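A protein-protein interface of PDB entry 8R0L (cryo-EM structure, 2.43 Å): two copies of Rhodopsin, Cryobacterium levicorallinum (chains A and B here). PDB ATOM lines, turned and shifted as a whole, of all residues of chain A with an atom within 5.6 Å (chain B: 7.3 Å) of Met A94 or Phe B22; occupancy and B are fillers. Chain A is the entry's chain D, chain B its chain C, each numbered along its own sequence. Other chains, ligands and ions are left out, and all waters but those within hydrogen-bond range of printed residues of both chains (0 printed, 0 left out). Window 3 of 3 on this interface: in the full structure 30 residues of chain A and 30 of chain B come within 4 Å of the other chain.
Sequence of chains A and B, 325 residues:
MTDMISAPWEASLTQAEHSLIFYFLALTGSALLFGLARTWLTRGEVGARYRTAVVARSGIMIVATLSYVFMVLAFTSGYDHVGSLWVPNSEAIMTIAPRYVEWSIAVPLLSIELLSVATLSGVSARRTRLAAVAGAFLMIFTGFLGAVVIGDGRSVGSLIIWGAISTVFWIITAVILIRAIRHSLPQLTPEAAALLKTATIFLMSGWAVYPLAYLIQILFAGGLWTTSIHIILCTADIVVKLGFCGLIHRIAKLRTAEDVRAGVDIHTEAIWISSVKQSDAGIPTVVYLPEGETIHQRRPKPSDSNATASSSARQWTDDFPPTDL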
ATOM      1  N   PHE A  70      -7.909   0.753 -15.054  1.00  0.00           N
ATOM      2  CA  PHE A  70      -9.202   0.120 -15.002  1.00  0.00           C
ATOM      3  C   PHE A  70     -10.288   1.184 -14.922  1.00  0.00           C
ATOM      4  O   PHE A  70     -11.338   1.048 -15.547  1.00  0.00           O
ATOM      5  CB  PHE A  70      -9.285  -0.788 -13.781  1.00  0.00           C
ATOM      6  CG  PHE A  70     -10.583  -1.532 -13.636  1.00  0.00           C
ATOM      7  CD1 PHE A  70     -10.787  -2.738 -14.291  1.00  0.00           C
ATOM      8  CD2 PHE A  70     -11.611  -1.016 -12.861  1.00  0.00           C
ATOM      9  CE1 PHE A  70     -11.983  -3.429 -14.150  1.00  0.00           C
ATOM     10  CE2 PHE A  70     -12.808  -1.712 -12.713  1.00  0.00           C
ATOM     11  CZ  PHE A  70     -12.994  -2.910 -13.365  1.00  0.00           C
ATOM     12  N   MET A  71     -10.033   2.227 -14.132  1.00  0.00           N
ATOM     13  CA  MET A  71     -11.027   3.245 -13.859  1.00  0.00           C
ATOM     14  C   MET A  71     -11.250   4.077 -15.109  1.00  0.00           C
ATOM     15  O   MET A  71     -12.367   4.456 -15.387  1.00  0.00           O
ATOM     16  CB  MET A  71     -10.595   4.142 -12.700  1.00  0.00           C
ATOM     17  CG  MET A  71     -10.954   3.566 -11.363  1.00  0.00           C
ATOM     18  SD  MET A  71     -10.658   4.749 -10.033  1.00  0.00           S
ATOM     19  CE  MET A  71      -8.904   4.484  -9.768  1.00  0.00           C
ATOM     20  N   ALA A  74     -13.199   1.983 -17.324  1.00  0.00           N
ATOM     21  CA  ALA A  74     -14.550   1.883 -16.792  1.00  0.00           C
ATOM     22  C   ALA A  74     -15.318   3.176 -17.044  1.00  0.00           C
ATOM     23  O   ALA A  74     -16.545   3.151 -17.125  1.00  0.00           O
ATOM     24  CB  ALA A  74     -14.559   1.577 -15.317  1.00  0.00           C
ATOM     25  N   SER A  90     -24.316   0.806 -14.992  1.00  0.00           N
ATOM     26  CA  SER A  90     -23.998  -0.071 -13.870  1.00  0.00           C
ATOM     27  C   SER A  90     -22.487  -0.196 -13.688  1.00  0.00           C
ATOM     28  O   SER A  90     -22.054  -0.696 -12.658  1.00  0.00           O
ATOM     29  CB  SER A  90     -24.649  -1.435 -14.035  1.00  0.00           C
ATOM     30  OG  SER A  90     -24.209  -2.077 -15.230  1.00  0.00           O
ATOM     31  N   GLU A  91     -21.704   0.246 -14.681  1.00  0.00           N
ATOM     32  CA  GLU A  91     -20.252   0.157 -14.622  1.00  0.00           C
ATOM     33  C   GLU A  91     -19.649   1.469 -14.109  1.00  0.00           C
ATOM     34  O   GLU A  91     -18.427   1.590 -14.040  1.00  0.00           O
ATOM     35  CB  GLU A  91     -19.685  -0.231 -15.993  1.00  0.00           C
ATOM     36  N   ALA A  92     -20.495   2.440 -13.733  1.00  0.00           N
ATOM     37  CA  ALA A  92     -20.021   3.696 -13.163  1.00  0.00           C
ATOM     38  C   ALA A  92     -19.486   3.477 -11.738  1.00  0.00           C
ATOM     39  O   ALA A  92     -18.554   4.177 -11.349  1.00  0.00           O
ATOM     40  CB  ALA A  92     -21.100   4.753 -13.228  1.00  0.00           C
ATOM     41  N   ILE A  93     -19.984   2.485 -10.985  1.00  0.00           N
ATOM     42  CA  ILE A  93     -19.416   2.215  -9.664  1.00  0.00           C
ATOM     43  C   ILE A  93     -17.949   1.769  -9.801  1.00  0.00           C
ATOM     44  O   ILE A  93     -17.166   1.891  -8.864  1.00  0.00           O
ATOM     45  CB  ILE A  93     -20.258   1.186  -8.878  1.00  0.00           C
ATOM     46  CG1 ILE A  93     -19.892   1.161  -7.399  1.00  0.00           C
ATOM     47  CG2 ILE A  93     -20.136  -0.195  -9.486  1.00  0.00           C
ATOM     48  CD1 ILE A  93     -20.877   0.404  -6.553  1.00  0.00           C
ATOM     49  N   MET A  94     -17.593   1.251 -10.976  1.00  0.00           N
ATOM     50  CA  MET A  94     -16.241   0.825 -11.279  1.00  0.00           C
ATOM     51  C   MET A  94     -15.328   2.016 -11.540  1.00  0.00           C
ATOM     52  O   MET A  94     -14.140   1.825 -11.775  1.00  0.00           O
ATOM     53  CB  MET A  94     -16.217  -0.074 -12.523  1.00  0.00           C
ATOM     54  CG  MET A  94     -16.628  -1.514 -12.245  1.00  0.00           C
ATOM     55  SD  MET A  94     -15.911  -2.197 -10.717  1.00  0.00           S
ATOM     56  CE  MET A  94     -17.385  -2.695  -9.817  1.00  0.00           C
ATOM     57  N   THR A  95     -15.880   3.228 -11.567  1.00  0.00           N
ATOM     58  CA  THR A  95     -15.054   4.421 -11.656  1.00  0.00           C
ATOM     59  C   THR A  95     -14.635   4.878 -10.259  1.00  0.00           C
ATOM     60  O   THR A  95     -13.739   5.702 -10.137  1.00  0.00           O
ATOM     61  CB  THR A  95     -15.782   5.558 -12.382  1.00  0.00           C
ATOM     62  OG1 THR A  95     -16.945   5.885 -11.617  1.00  0.00           O
ATOM     63  CG2 THR A  95     -16.141   5.196 -13.806  1.00  0.00           C
ATOM     64  N   ILE A  96     -15.313   4.401  -9.219  1.00  0.00           N
ATOM     65  CA  ILE A  96     -15.036   4.854  -7.875  1.00  0.00           C
ATOM     66  C   ILE A  96     -14.490   3.718  -7.007  1.00  0.00           C
ATOM     67  O   ILE A  96     -13.648   3.958  -6.153  1.00  0.00           O
ATOM     68  CB  ILE A  96     -16.312   5.486  -7.284  1.00  0.00           C
ATOM     69  CG1 ILE A  96     -16.577   6.861  -7.906  1.00  0.00           C
ATOM     70  CG2 ILE A  96     -16.281   5.527  -5.757  1.00  0.00           C
ATOM     71  CD1 ILE A  96     -15.711   7.974  -7.360  1.00  0.00           C
ATOM     72  N   ALA A  97     -14.967   2.488  -7.191  1.00  0.00           N
ATOM     73  CA  ALA A  97     -14.678   1.408  -6.254  1.00  0.00           C
ATOM     74  C   ALA A  97     -13.242   0.891  -6.343  1.00  0.00           C
ATOM     75  O   ALA A  97     -12.694   0.480  -5.329  1.00  0.00           O
ATOM     76  CB  ALA A  97     -15.672   0.293  -6.439  1.00  0.00           C
ATOM     77  N   PRO A  98     -12.578   0.843  -7.509  1.00  0.00           N
ATOM     78  CA  PRO A  98     -11.194   0.367  -7.581  1.00  0.00           C
ATOM     79  C   PRO A  98     -10.220   1.161  -6.711  1.00  0.00           C
ATOM     80  O   PRO A  98      -9.155   0.662  -6.380  1.00  0.00           O
ATOM     81  CB  PRO A  98     -10.830   0.502  -9.070  1.00  0.00           C
ATOM     82  CG  PRO A  98     -12.183   0.455  -9.763  1.00  0.00           C
ATOM     83  CD  PRO A  98     -13.113   1.202  -8.822  1.00  0.00           C
ATOM     84  N   VAL A 101      -9.508  -0.660  -3.659  1.00  0.00           N
ATOM     85  CA  VAL A 101      -8.640  -1.799  -3.883  1.00  0.00           C
ATOM     86  C   VAL A 101      -7.200  -1.334  -3.848  1.00  0.00           C
ATOM     87  O   VAL A 101      -6.373  -1.987  -3.225  1.00  0.00           O
ATOM     88  CB  VAL A 101      -8.938  -2.522  -5.208  1.00  0.00           C
ATOM     89  CG1 VAL A 101      -7.934  -3.635  -5.476  1.00  0.00           C
ATOM     90  CG2 VAL A 101     -10.359  -3.060  -5.225  1.00  0.00           C
ATOM     91  N   ALA B  16     -24.301  -6.071  -2.670  1.00  0.00           N
ATOM     92  CA  ALA B  16     -23.249  -6.167  -1.673  1.00  0.00           C
ATOM     93  C   ALA B  16     -22.288  -7.297  -2.026  1.00  0.00           C
ATOM     94  O   ALA B  16     -21.075  -7.095  -2.045  1.00  0.00           O
ATOM     95  CB  ALA B  16     -23.801  -6.355  -0.299  1.00  0.00           C
ATOM     96  N   GLU B  17     -22.845  -8.473  -2.310  1.00  0.00           N
ATOM     97  CA  GLU B  17     -22.065  -9.628  -2.689  1.00  0.00           C
ATOM     98  C   GLU B  17     -21.295  -9.334  -3.961  1.00  0.00           C
ATOM     99  O   GLU B  17     -20.142  -9.715  -4.078  1.00  0.00           O
ATOM    100  CB  GLU B  17     -22.977 -10.844  -2.864  1.00  0.00           C
ATOM    101  CG  GLU B  17     -23.589 -11.324  -1.549  1.00  0.00           C
ATOM    102  CD  GLU B  17     -24.902 -12.090  -1.729  1.00  0.00           C
ATOM    103  OE1 GLU B  17     -25.458 -12.604  -0.714  1.00  0.00           O
ATOM    104  OE2 GLU B  17     -25.397 -12.191  -2.893  1.00  0.00           O
ATOM    105  N   HIS B  18     -21.931  -8.701  -4.929  1.00  0.00           N
ATOM    106  CA  HIS B  18     -21.285  -8.455  -6.208  1.00  0.00           C
ATOM    107  C   HIS B  18     -20.083  -7.539  -5.990  1.00  0.00           C
ATOM    108  O   HIS B  18     -19.053  -7.677  -6.660  1.00  0.00           O
ATOM    109  CB  HIS B  18     -22.305  -7.872  -7.189  1.00  0.00           C
ATOM    110  CG  HIS B  18     -21.820  -7.709  -8.573  1.00  0.00           C
ATOM    111  ND1 HIS B  18     -21.338  -6.504  -9.038  1.00  0.00           N
ATOM    112  CD2 HIS B  18     -21.662  -8.631  -9.568  1.00  0.00           C
ATOM    113  CE1 HIS B  18     -20.916  -6.689 -10.300  1.00  0.00           C
ATOM    114  NE2 HIS B  18     -21.096  -7.975 -10.648  1.00  0.00           N
ATOM    115  N   SER B  19     -20.254  -6.603  -5.052  1.00  0.00           N
ATOM    116  CA  SER B  19     -19.248  -5.614  -4.743  1.00  0.00           C
ATOM    117  C   SER B  19     -18.094  -6.237  -3.975  1.00  0.00           C
ATOM    118  O   SER B  19     -16.933  -6.025  -4.339  1.00  0.00           O
ATOM    119  CB  SER B  19     -19.868  -4.443  -4.001  1.00  0.00           C
ATOM    120  OG  SER B  19     -20.292  -3.432  -4.941  1.00  0.00           O
ATOM    121  N   LEU B  20     -18.433  -7.022  -2.945  1.00  0.00           N
ATOM    122  CA  LEU B  20     -17.437  -7.797  -2.234  1.00  0.00           C
ATOM    123  C   LEU B  20     -16.645  -8.739  -3.158  1.00  0.00           C
ATOM    124  O   LEU B  20     -15.439  -8.845  -3.027  1.00  0.00           O
ATOM    125  CB  LEU B  20     -18.122  -8.528  -1.100  1.00  0.00           C
ATOM    126  CG  LEU B  20     -18.259  -7.711   0.170  1.00  0.00           C
ATOM    127  CD1 LEU B  20     -19.023  -8.508   1.195  1.00  0.00           C
ATOM    128  CD2 LEU B  20     -16.907  -7.331   0.732  1.00  0.00           C
ATOM    129  N   ILE B  21     -17.250  -9.361  -4.152  1.00  0.00           N
ATOM    130  CA  ILE B  21     -16.497 -10.313  -4.951  1.00  0.00           C
ATOM    131  C   ILE B  21     -15.534  -9.600  -5.882  1.00  0.00           C
ATOM    132  O   ILE B  21     -14.465 -10.133  -6.162  1.00  0.00           O
ATOM    133  CB  ILE B  21     -17.409 -11.284  -5.714  1.00  0.00           C
ATOM    134  CG1 ILE B  21     -18.186 -12.165  -4.740  1.00  0.00           C
ATOM    135  CG2 ILE B  21     -16.604 -12.106  -6.711  1.00  0.00           C
ATOM    136  CD1 ILE B  21     -19.289 -12.956  -5.376  1.00  0.00           C
ATOM    137  N   PHE B  22     -15.934  -8.452  -6.432  1.00  0.00           N
ATOM    138  CA  PHE B  22     -15.049  -7.660  -7.272  1.00  0.00           C
ATOM    139  C   PHE B  22     -13.852  -7.204  -6.436  1.00  0.00           C
ATOM    140  O   PHE B  22     -12.712  -7.251  -6.895  1.00  0.00           O
ATOM    141  CB  PHE B  22     -15.776  -6.431  -7.842  1.00  0.00           C
ATOM    142  CG  PHE B  22     -14.841  -5.345  -8.325  1.00  0.00           C
ATOM    143  CD1 PHE B  22     -14.251  -5.426  -9.585  1.00  0.00           C
ATOM    144  CD2 PHE B  22     -14.454  -4.308  -7.475  1.00  0.00           C
ATOM    145  CE1 PHE B  22     -13.314  -4.478  -9.985  1.00  0.00           C
ATOM    146  CE2 PHE B  22     -13.520  -3.363  -7.881  1.00  0.00           C
ATOM    147  CZ  PHE B  22     -12.947  -3.448  -9.134  1.00  0.00           C
ATOM    148  N   TYR B  23     -14.123  -6.776  -5.201  1.00  0.00           N
ATOM    149  CA  TYR B  23     -13.069  -6.254  -4.365  1.00  0.00           C
ATOM    150  C   TYR B  23     -11.977  -7.300  -4.162  1.00  0.00           C
ATOM    151  O   TYR B  23     -10.827  -7.087  -4.563  1.00  0.00           O
ATOM    152  CB  TYR B  23     -13.701  -5.845  -3.051  1.00  0.00           C
ATOM    153  CG  TYR B  23     -12.712  -5.325  -2.041  1.00  0.00           C
ATOM    154  CD1 TYR B  23     -12.217  -4.017  -2.109  1.00  0.00           C
ATOM    155  CD2 TYR B  23     -12.247  -6.155  -1.029  1.00  0.00           C
ATOM    156  CE1 TYR B  23     -11.325  -3.536  -1.160  1.00  0.00           C
ATOM    157  CE2 TYR B  23     -11.347  -5.685  -0.077  1.00  0.00           C
ATOM    158  CZ  TYR B  23     -10.888  -4.379  -0.147  1.00  0.00           C
ATOM    159  OH  TYR B  23      -9.989  -4.006   0.799  1.00  0.00           O
ATOM    160  N   PHE B  24     -12.377  -8.453  -3.609  1.00  0.00           N
ATOM    161  CA  PHE B  24     -11.473  -9.525  -3.272  1.00  0.00           C
ATOM    162  C   PHE B  24     -10.795 -10.056  -4.526  1.00  0.00           C
ATOM    163  O   PHE B  24      -9.613 -10.378  -4.510  1.00  0.00           O
ATOM    164  CB  PHE B  24     -12.229 -10.565  -2.467  1.00  0.00           C
ATOM    165  CG  PHE B  24     -12.354 -10.225  -1.007  1.00  0.00           C
ATOM    166  CD1 PHE B  24     -11.326 -10.511  -0.127  1.00  0.00           C
ATOM    167  CD2 PHE B  24     -13.488  -9.614  -0.511  1.00  0.00           C
ATOM    168  CE1 PHE B  24     -11.430 -10.181   1.218  1.00  0.00           C
ATOM    169  CE2 PHE B  24     -13.594  -9.294   0.840  1.00  0.00           C
ATOM    170  CZ  PHE B  24     -12.564  -9.566   1.701  1.00  0.00           C
ATOM    171  N   LEU B  25     -11.497 -10.125  -5.632  1.00  0.00           N
ATOM    172  CA  LEU B  25     -10.837 -10.608  -6.825  1.00  0.00           C
ATOM    173  C   LEU B  25      -9.754  -9.648  -7.285  1.00  0.00           C
ATOM    174  O   LEU B  25      -8.718 -10.076  -7.760  1.00  0.00           O
ATOM    175  CB  LEU B  25     -11.865 -10.787  -7.931  1.00  0.00           C
ATOM    176  CG  LEU B  25     -12.707 -12.052  -7.887  1.00  0.00           C
ATOM    177  CD1 LEU B  25     -13.554 -12.068  -9.154  1.00  0.00           C
ATOM    178  CD2 LEU B  25     -11.856 -13.302  -7.774  1.00  0.00           C
ATOM    179  N   ALA B  26     -10.028  -8.356  -7.209  1.00  0.00           N
ATOM    180  CA  ALA B  26      -9.096  -7.316  -7.634  1.00  0.00           C
ATOM    181  C   ALA B  26      -7.984  -7.117  -6.596  1.00  0.00           C
ATOM    182  O   ALA B  26      -6.852  -6.827  -6.974  1.00  0.00           O
ATOM    183  CB  ALA B  26      -9.876  -6.045  -7.879  1.00  0.00           C
ATOM    184  N   LEU B  27      -8.311  -7.282  -5.308  1.00  0.00           N
ATOM    185  CA  LEU B  27      -7.309  -7.238  -4.259  1.00  0.00           C
ATOM    186  C   LEU B  27      -6.259  -8.331  -4.450  1.00  0.00           C
ATOM    187  O   LEU B  27      -5.085  -8.108  -4.187  1.00  0.00           O
ATOM    188  CB  LEU B  27      -7.987  -7.415  -2.911  1.00  0.00           C
ATOM    189  CG  LEU B  27      -7.099  -7.145  -1.714  1.00  0.00           C
ATOM    190  CD1 LEU B  27      -6.783  -5.657  -1.596  1.00  0.00           C
ATOM    191  CD2 LEU B  27      -7.795  -7.658  -0.457  1.00  0.00           C
ATOM    192  N   THR B  28      -6.697  -9.510  -4.884  1.00  0.00           N
ATOM    193  CA  THR B  28      -5.817 -10.640  -5.048  1.00  0.00           C
ATOM    194  C   THR B  28      -4.952 -10.413  -6.271  1.00  0.00           C
ATOM    195  O   THR B  28      -3.755 -10.642  -6.201  1.00  0.00           O
ATOM    196  CB  THR B  28      -6.627 -11.933  -5.040  1.00  0.00           C
ATOM    197  OG1 THR B  28      -7.466 -11.772  -3.896  1.00  0.00           O
ATOM    198  CG2 THR B  28      -5.783 -13.181  -4.908  1.00  0.00           C
ATOM    199  N   VAL B  72     -11.333 -11.264 -13.110  1.00  0.00           N
ATOM    200  CA  VAL B  72     -11.914  -9.970 -12.802  1.00  0.00           C
ATOM    201  C   VAL B  72     -12.610  -9.421 -14.043  1.00  0.00           C
ATOM    202  O   VAL B  72     -13.661  -8.802 -13.932  1.00  0.00           O
ATOM    203  CB  VAL B  72     -10.855  -8.993 -12.262  1.00  0.00           C
ATOM    204  CG1 VAL B  72     -11.194  -7.542 -12.557  1.00  0.00           C
ATOM    205  CG2 VAL B  72     -10.647  -9.193 -10.772  1.00  0.00           C
ATOM    206  N   PHE B  75     -15.674 -11.406 -14.601  1.00  0.00           N
ATOM    207  CA  PHE B  75     -16.687 -11.078 -13.619  1.00  0.00           C
ATOM    208  C   PHE B  75     -17.489  -9.903 -14.158  1.00  0.00           C
ATOM    209  O   PHE B  75     -18.706  -9.851 -13.995  1.00  0.00           O
ATOM    210  CB  PHE B  75     -16.038 -10.765 -12.265  1.00  0.00           C
ATOM    211  CG  PHE B  75     -16.981 -10.565 -11.102  1.00  0.00           C
ATOM    212  CD1 PHE B  75     -17.606 -11.647 -10.494  1.00  0.00           C
ATOM    213  CD2 PHE B  75     -17.255  -9.299 -10.621  1.00  0.00           C
ATOM    214  CE1 PHE B  75     -18.479 -11.471  -9.430  1.00  0.00           C
ATOM    215  CE2 PHE B  75     -18.111  -9.127  -9.542  1.00  0.00           C
ATOM    216  CZ  PHE B  75     -18.731 -10.210  -8.959  1.00  0.00           C
ATOM    217  N   THR B  76     -16.789  -8.971 -14.802  1.00  0.00           N
ATOM    218  CA  THR B  76     -17.423  -7.783 -15.346  1.00  0.00           C
ATOM    219  C   THR B  76     -18.397  -8.209 -16.444  1.00  0.00           C
ATOM    220  O   THR B  76     -19.485  -7.649 -16.550  1.00  0.00           O
ATOM    221  CB  THR B  76     -16.366  -6.768 -15.807  1.00  0.00           C
ATOM    222  OG1 THR B  76     -15.463  -7.415 -16.708  1.00  0.00           O
ATOM    223  CG2 THR B  76     -15.589  -6.167 -14.652  1.00  0.00           C
ATOM    224  N   TRP B  86     -27.589  -9.293  -9.215  1.00  0.00           N
ATOM    225  CA  TRP B  86     -26.756  -9.515 -10.372  1.00  0.00           C
ATOM    226  C   TRP B  86     -26.952 -10.950 -10.828  1.00  0.00           C
ATOM    227  O   TRP B  86     -26.945 -11.870 -10.013  1.00  0.00           O
ATOM    228  CB  TRP B  86     -25.299  -9.192 -10.058  1.00  0.00           C
ATOM    229  CG  TRP B  86     -25.049  -7.724  -9.906  1.00  0.00           C
ATOM    230  CD1 TRP B  86     -25.248  -6.933  -8.816  1.00  0.00           C
ATOM    231  CD2 TRP B  86     -24.459  -6.885 -10.909  1.00  0.00           C
ATOM    232  NE1 TRP B  86     -24.842  -5.646  -9.088  1.00  0.00           N
ATOM    233  CE2 TRP B  86     -24.344  -5.605 -10.357  1.00  0.00           C
ATOM    234  CE3 TRP B  86     -24.011  -7.115 -12.205  1.00  0.00           C
ATOM    235  CZ2 TRP B  86     -23.799  -4.548 -11.061  1.00  0.00           C
ATOM    236  CZ3 TRP B  86     -23.447  -6.070 -12.894  1.00  0.00           C
ATOM    237  CH2 TRP B  86     -23.335  -4.804 -12.330  1.00  0.00           C
ATOM    238  N   HIS B 230     -15.388 -17.172  -2.664  1.00  0.00           N
ATOM    239  CA  HIS B 230     -14.470 -16.275  -3.325  1.00  0.00           C
ATOM    240  C   HIS B 230     -13.542 -15.632  -2.307  1.00  0.00           C
ATOM    241  O   HIS B 230     -12.371 -15.406  -2.589  1.00  0.00           O
ATOM    242  CB  HIS B 230     -15.264 -15.212  -4.075  1.00  0.00           C
ATOM    243  CG  HIS B 230     -15.563 -15.575  -5.468  1.00  0.00           C
ATOM    244  ND1 HIS B 230     -16.814 -15.920  -5.909  1.00  0.00           N
ATOM    245  CD2 HIS B 230     -14.750 -15.639  -6.532  1.00  0.00           C
ATOM    246  CE1 HIS B 230     -16.737 -16.170  -7.211  1.00  0.00           C
ATOM    247  NE2 HIS B 230     -15.488 -16.031  -7.613  1.00  0.00           N
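CZ of Phe A70 touches CE1 of Phe B22, 3.7 Å away. Ser A90 touches Trp B86 (CB to CH2, 3.998 Å). Met A94 touches Phe B22. CD1 of Tyr B23 touches CG2 of Val A101, at 3.8 Å. Ala B26 touches Val A101. Val A101 touches Leu B27 (CG1 to N, 3.7 Å).
Printed residues of chain B within 4 Å of Met A94: Phe B22 (3.5 Å). Phe B22 touches two residues of chain A. Of the printed residues of chain B, Phe A70 touches Phe B22 (3.7 Å). Of the printed residues of chain A, Trp B86 touches Ser A90. Ala A92 touches none of the printed residues of chain B. Ser B19 touches none of the printed residues of chain A. The nearest residue of chain A that does not touch Phe B22 is Pro A98 (4.03 Å). The nearest printed residue of chain B that does not touch Ser A90 is His B18 (6.5 Å).
Printed residues of chain A that touch a printed residue of chain B: Phe A70, Ser A90, Met A94 and Val A101. Hydrophobic or aromatic side chains of chain A within 4 Å of the printed part of chain B: Phe A70, Met A94 and Val A101.
No position is printed for both chains. Of the 6 pairs that touch across the chains among the printed residues, none has its exchanged pair printed and touching as well.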
